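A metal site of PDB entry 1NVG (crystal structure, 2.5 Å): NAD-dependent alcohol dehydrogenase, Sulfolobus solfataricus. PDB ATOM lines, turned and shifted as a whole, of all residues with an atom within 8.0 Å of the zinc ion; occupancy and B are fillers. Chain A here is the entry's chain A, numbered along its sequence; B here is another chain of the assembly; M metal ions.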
ATOM      1  N   GLN A  96     -17.829  30.590 -28.832  1.00  0.00           N
ATOM      2  CA  GLN A  96     -17.735  29.188 -29.226  1.00  0.00           C
ATOM      3  C   GLN A  96     -18.032  28.169 -28.134  1.00  0.00           C
ATOM      4  O   GLN A  96     -17.756  28.410 -26.958  1.00  0.00           O
ATOM      5  CB  GLN A  96     -16.349  28.954 -29.822  1.00  0.00           C
ATOM      6  CG  GLN A  96     -15.983  30.035 -30.837  1.00  0.00           C
ATOM      7  CD  GLN A  96     -14.635  29.795 -31.481  1.00  0.00           C
ATOM      8  OE1 GLN A  96     -13.824  29.007 -30.989  1.00  0.00           O
ATOM      9  NE2 GLN A  96     -14.384  30.471 -32.599  1.00  0.00           N
ATOM     10  N   GLY A  97     -18.608  27.043 -28.534  1.00  0.00           N
ATOM     11  CA  GLY A  97     -18.942  25.987 -27.597  1.00  0.00           C
ATOM     12  C   GLY A  97     -18.092  24.748 -27.790  1.00  0.00           C
ATOM     13  O   GLY A  97     -17.384  24.614 -28.792  1.00  0.00           O
ATOM     14  N   GLU A  98     -18.143  23.822 -26.831  1.00  0.00           N
ATOM     15  CA  GLU A  98     -17.295  22.651 -26.954  1.00  0.00           C
ATOM     16  C   GLU A  98     -17.940  21.533 -27.768  1.00  0.00           C
ATOM     17  O   GLU A  98     -17.230  20.697 -28.327  1.00  0.00           O
ATOM     18  CB  GLU A  98     -16.873  22.186 -25.560  1.00  0.00           C
ATOM     19  CG  GLU A  98     -17.946  22.175 -24.509  1.00  0.00           C
ATOM     20  CD  GLU A  98     -19.030  21.159 -24.820  1.00  0.00           C
ATOM     21  OE1 GLU A  98     -18.728  20.126 -25.457  1.00  0.00           O
ATOM     22  OE2 GLU A  98     -20.190  21.391 -24.405  1.00  0.00           O
ATOM     23  N   GLY A  99     -19.272  21.529 -27.841  1.00  0.00           N
ATOM     24  CA  GLY A  99     -19.970  20.615 -28.747  1.00  0.00           C
ATOM     25  C   GLY A  99     -20.853  19.533 -28.139  1.00  0.00           C
ATOM     26  O   GLY A  99     -21.870  19.143 -28.705  1.00  0.00           O
ATOM     27  N   ASN A 100     -20.452  19.076 -26.959  1.00  0.00           N
ATOM     28  CA  ASN A 100     -21.077  17.948 -26.289  1.00  0.00           C
ATOM     29  C   ASN A 100     -22.285  18.251 -25.414  1.00  0.00           C
ATOM     30  O   ASN A 100     -23.165  17.384 -25.242  1.00  0.00           O
ATOM     31  CB  ASN A 100     -20.025  17.253 -25.426  1.00  0.00           C
ATOM     32  CG  ASN A 100     -20.543  15.985 -24.808  1.00  0.00           C
ATOM     33  OD1 ASN A 100     -20.950  15.068 -25.510  1.00  0.00           O
ATOM     34  ND2 ASN A 100     -20.535  15.922 -23.474  1.00  0.00           N
ATOM     35  N   CYS A 101     -22.336  19.448 -24.835  1.00  0.00           N
ATOM     36  CA  CYS A 101     -23.435  19.795 -23.928  1.00  0.00           C
ATOM     37  C   CYS A 101     -24.788  20.034 -24.622  1.00  0.00           C
ATOM     38  O   CYS A 101     -24.877  20.080 -25.869  1.00  0.00           O
ATOM     39  CB  CYS A 101     -23.064  21.014 -23.056  1.00  0.00           C
ATOM     40  SG  CYS A 101     -23.207  22.669 -23.828  1.00  0.00           S
ATOM     41  N   TYR A 102     -25.825  20.169 -23.808  1.00  0.00           N
ATOM     42  CA  TYR A 102     -27.172  20.418 -24.287  1.00  0.00           C
ATOM     43  C   TYR A 102     -27.206  21.595 -25.279  1.00  0.00           C
ATOM     44  O   TYR A 102     -27.558  21.445 -26.446  1.00  0.00           O
ATOM     45  CB  TYR A 102     -28.091  20.725 -23.097  1.00  0.00           C
ATOM     46  CG  TYR A 102     -29.481  21.105 -23.505  1.00  0.00           C
ATOM     47  CD1 TYR A 102     -30.372  20.151 -23.988  1.00  0.00           C
ATOM     48  CD2 TYR A 102     -29.908  22.434 -23.438  1.00  0.00           C
ATOM     49  CE1 TYR A 102     -31.657  20.512 -24.410  1.00  0.00           C
ATOM     50  CE2 TYR A 102     -31.188  22.811 -23.852  1.00  0.00           C
ATOM     51  CZ  TYR A 102     -32.056  21.834 -24.342  1.00  0.00           C
ATOM     52  OH  TYR A 102     -33.305  22.191 -24.791  1.00  0.00           O
ATOM     53  N   TYR A 103     -26.799  22.757 -24.791  1.00  0.00           N
ATOM     54  CA  TYR A 103     -26.821  23.962 -25.595  1.00  0.00           C
ATOM     55  C   TYR A 103     -26.077  23.825 -26.897  1.00  0.00           C
ATOM     56  O   TYR A 103     -26.558  24.320 -27.922  1.00  0.00           O
ATOM     57  CB  TYR A 103     -26.324  25.132 -24.755  1.00  0.00           C
ATOM     58  CG  TYR A 103     -27.209  25.308 -23.561  1.00  0.00           C
ATOM     59  CD1 TYR A 103     -28.495  25.857 -23.703  1.00  0.00           C
ATOM     60  CD2 TYR A 103     -26.858  24.793 -22.324  1.00  0.00           C
ATOM     61  CE1 TYR A 103     -29.406  25.867 -22.632  1.00  0.00           C
ATOM     62  CE2 TYR A 103     -27.754  24.806 -21.240  1.00  0.00           C
ATOM     63  CZ  TYR A 103     -29.037  25.335 -21.412  1.00  0.00           C
ATOM     64  OH  TYR A 103     -29.958  25.288 -20.380  1.00  0.00           O
ATOM     65  N   CYS A 104     -24.949  23.118 -26.895  1.00  0.00           N
ATOM     66  CA  CYS A 104     -24.218  22.917 -28.150  1.00  0.00           C
ATOM     67  C   CYS A 104     -25.006  21.974 -29.051  1.00  0.00           C
ATOM     68  O   CYS A 104     -25.117  22.216 -30.250  1.00  0.00           O
ATOM     69  CB  CYS A 104     -22.798  22.356 -27.898  1.00  0.00           C
ATOM     70  SG  CYS A 104     -21.568  23.496 -27.137  1.00  0.00           S
ATOM     71  N   ARG A 105     -25.562  20.892 -28.508  1.00  0.00           N
ATOM     72  CA  ARG A 105     -26.312  19.977 -29.365  1.00  0.00           C
ATOM     73  C   ARG A 105     -27.579  20.623 -29.969  1.00  0.00           C
ATOM     74  O   ARG A 105     -27.974  20.286 -31.105  1.00  0.00           O
ATOM     75  CB  ARG A 105     -26.700  18.710 -28.619  1.00  0.00           C
ATOM     76  CG  ARG A 105     -25.534  17.902 -28.112  1.00  0.00           C
ATOM     77  CD  ARG A 105     -26.002  16.634 -27.411  1.00  0.00           C
ATOM     78  NE  ARG A 105     -24.898  15.948 -26.759  1.00  0.00           N
ATOM     79  CZ  ARG A 105     -24.657  14.636 -26.857  1.00  0.00           C
ATOM     80  NH1 ARG A 105     -25.456  13.863 -27.590  1.00  0.00           N
ATOM     81  NH2 ARG A 105     -23.621  14.110 -26.220  1.00  0.00           N
ATOM     82  N   GLU A 108     -27.352  26.234 -29.714  1.00  0.00           N
ATOM     83  CA  GLU A 108     -27.158  27.447 -28.943  1.00  0.00           C
ATOM     84  C   GLU A 108     -25.739  27.485 -28.360  1.00  0.00           C
ATOM     85  O   GLU A 108     -25.561  27.673 -27.162  1.00  0.00           O
ATOM     86  CB  GLU A 108     -28.196  27.506 -27.822  1.00  0.00           C
ATOM     87  CG  GLU A 108     -29.631  27.423 -28.327  1.00  0.00           C
ATOM     88  CD  GLU A 108     -30.057  28.637 -29.131  1.00  0.00           C
ATOM     89  OE1 GLU A 108     -29.199  29.414 -29.594  1.00  0.00           O
ATOM     90  OE2 GLU A 108     -31.275  28.826 -29.325  1.00  0.00           O
ATOM     91  N   GLU A 109     -24.730  27.303 -29.224  1.00  0.00           N
ATOM     92  CA  GLU A 109     -23.323  27.217 -28.807  1.00  0.00           C
ATOM     93  C   GLU A 109     -22.922  28.281 -27.793  1.00  0.00           C
ATOM     94  O   GLU A 109     -22.226  27.999 -26.825  1.00  0.00           O
ATOM     95  CB  GLU A 109     -22.397  27.291 -30.028  1.00  0.00           C
ATOM     96  N   HIS A 110     -23.378  29.519 -28.006  1.00  0.00           N
ATOM     97  CA  HIS A 110     -22.990  30.603 -27.126  1.00  0.00           C
ATOM     98  C   HIS A 110     -23.382  30.405 -25.668  1.00  0.00           C
ATOM     99  O   HIS A 110     -22.836  31.066 -24.775  1.00  0.00           O
ATOM    100  CB  HIS A 110     -23.544  31.930 -27.638  1.00  0.00           C
ATOM    101  CG  HIS A 110     -25.027  32.049 -27.553  1.00  0.00           C
ATOM    102  ND1 HIS A 110     -25.888  31.223 -28.246  1.00  0.00           N
ATOM    103  CD2 HIS A 110     -25.811  32.941 -26.883  1.00  0.00           C
ATOM    104  CE1 HIS A 110     -27.132  31.599 -28.016  1.00  0.00           C
ATOM    105  NE2 HIS A 110     -27.114  32.631 -27.196  1.00  0.00           N
ATOM    106  N   LEU A 111     -24.299  29.473 -25.404  1.00  0.00           N
ATOM    107  CA  LEU A 111     -24.748  29.231 -24.028  1.00  0.00           C
ATOM    108  C   LEU A 111     -24.125  27.960 -23.468  1.00  0.00           C
ATOM    109  O   LEU A 111     -24.561  27.421 -22.442  1.00  0.00           O
ATOM    110  CB  LEU A 111     -26.274  29.160 -23.975  1.00  0.00           C
ATOM    111  CG  LEU A 111     -26.973  30.491 -24.262  1.00  0.00           C
ATOM    112  CD1 LEU A 111     -28.482  30.295 -24.362  1.00  0.00           C
ATOM    113  CD2 LEU A 111     -26.624  31.488 -23.169  1.00  0.00           C
ATOM    114  N   CYS A 112     -23.097  27.497 -24.166  1.00  0.00           N
ATOM    115  CA  CYS A 112     -22.340  26.311 -23.790  1.00  0.00           C
ATOM    116  C   CYS A 112     -21.975  26.265 -22.323  1.00  0.00           C
ATOM    117  O   CYS A 112     -21.622  27.285 -21.720  1.00  0.00           O
ATOM    118  CB  CYS A 112     -21.059  26.248 -24.617  1.00  0.00           C
ATOM    119  SG  CYS A 112     -20.000  24.877 -24.108  1.00  0.00           S
ATOM    120  N   ASP A 113     -22.057  25.064 -21.744  1.00  0.00           N
ATOM    121  CA  ASP A 113     -21.676  24.851 -20.339  1.00  0.00           C
ATOM    122  C   ASP A 113     -20.199  25.101 -20.052  1.00  0.00           C
ATOM    123  O   ASP A 113     -19.820  25.361 -18.910  1.00  0.00           O
ATOM    124  CB  ASP A 113     -22.009  23.425 -19.897  1.00  0.00           C
ATOM    125  CG  ASP A 113     -23.501  23.157 -19.810  1.00  0.00           C
ATOM    126  OD1 ASP A 113     -24.267  24.080 -19.474  1.00  0.00           O
ATOM    127  OD2 ASP A 113     -23.884  21.994 -20.071  1.00  0.00           O
ATOM    128  N   SER A 114     -19.357  25.013 -21.068  1.00  0.00           N
ATOM    129  CA  SER A 114     -17.918  25.248 -20.922  1.00  0.00           C
ATOM    130  C   SER A 114     -17.467  26.112 -22.105  1.00  0.00           C
ATOM    131  O   SER A 114     -16.705  25.684 -22.963  1.00  0.00           O
ATOM    132  CB  SER A 114     -17.169  23.915 -20.905  1.00  0.00           C
ATOM    133  OG  SER A 114     -17.599  23.112 -19.810  1.00  0.00           O
ATOM    134  N   PRO A 115     -17.937  27.365 -22.143  1.00  0.00           N
ATOM    135  CA  PRO A 115     -17.620  28.280 -23.235  1.00  0.00           C
ATOM    136  C   PRO A 115     -16.148  28.487 -23.588  1.00  0.00           C
ATOM    137  O   PRO A 115     -15.261  28.430 -22.729  1.00  0.00           O
ATOM    138  CB  PRO A 115     -18.294  29.582 -22.793  1.00  0.00           C
ATOM    139  CG  PRO A 115     -18.239  29.492 -21.303  1.00  0.00           C
ATOM    140  CD  PRO A 115     -18.620  28.066 -21.042  1.00  0.00           C
ATOM    141  N   ARG A 116     -15.915  28.711 -24.872  1.00  0.00           N
ATOM    142  CA  ARG A 116     -14.607  29.093 -25.382  1.00  0.00           C
ATOM    143  C   ARG A 116     -14.816  30.449 -26.022  1.00  0.00           C
ATOM    144  O   ARG A 116     -15.072  30.533 -27.215  1.00  0.00           O
ATOM    145  CB  ARG A 116     -14.136  28.093 -26.427  1.00  0.00           C
ATOM    146  CG  ARG A 116     -13.886  26.721 -25.850  1.00  0.00           C
ATOM    147  CD  ARG A 116     -13.669  25.664 -26.922  1.00  0.00           C
ATOM    148  NE  ARG A 116     -13.517  24.360 -26.287  1.00  0.00           N
ATOM    149  CZ  ARG A 116     -13.299  23.221 -26.941  1.00  0.00           C
ATOM    150  NH1 ARG A 116     -13.206  23.226 -28.275  1.00  0.00           N
ATOM    151  NH2 ARG A 116     -13.158  22.080 -26.266  1.00  0.00           N
ATOM    152  N   LYS B 263     -30.453  27.631 -18.293  1.00  0.00           N
ATOM    153  CA  LYS B 263     -30.333  28.684 -19.286  1.00  0.00           C
ATOM    154  C   LYS B 263     -31.478  28.539 -20.310  1.00  0.00           C
ATOM    155  O   LYS B 263     -31.912  27.425 -20.616  1.00  0.00           O
ATOM    156  CB  LYS B 263     -28.959  28.597 -19.965  1.00  0.00           C
ATOM    157  CG  LYS B 263     -27.836  29.136 -19.066  1.00  0.00           C
ATOM    158  CD  LYS B 263     -26.443  28.789 -19.582  1.00  0.00           C
ATOM    159  CE  LYS B 263     -26.089  27.322 -19.320  1.00  0.00           C
ATOM    160  NZ  LYS B 263     -24.793  26.916 -19.944  1.00  0.00           N
HETATM  161 ZN    ZN M   1     -21.312  23.129 -24.967  1.00  0.00          ZN
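The side-chain carboxylate (OE1) of Glu 98 lies within hydrogen-bond range of the backbone NH (N) of Asn 100, at 2.5 Å. The side-chain sulfur (SG) of Cys 104 lies close to the backbone NH (N) of Gly 99 (3.1 Å). SG of Cys 101 sits close to N of Asp 113, at 3.4 Å. SG of Cys 101 sits close to N of Tyr 103, at 3.7 Å. The backbone NH (N) of Ser 114 sits close to the side-chain sulfur (SG) of Cys 112 (3.1 Å). The side-chain amino group of Lys 263 of chain B is in salt-bridge range of the side-chain carboxylate of Asp 113 (2.9 Å).
Merely in contact with the zinc ion: Gly 99 and Asp 113. Six residues have an atom within 4 Å of the zinc ion: Glu 98, Gly 99, Cys 101, Cys 104, Cys 112 and Asp 113. The nearest printed residue that does not touch the zinc ion is Gly 97 (4.5 Å).
The zinc ion is bound by OE2 of Glu 98 (2.1 Å). The zinc ion is bound by SG of Cys 104 (2.2 Å). The zinc ion is bound by SG of Cys 101 (2.3 Å). SG of Cys 112 is bound to the zinc ion (2.3 Å).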
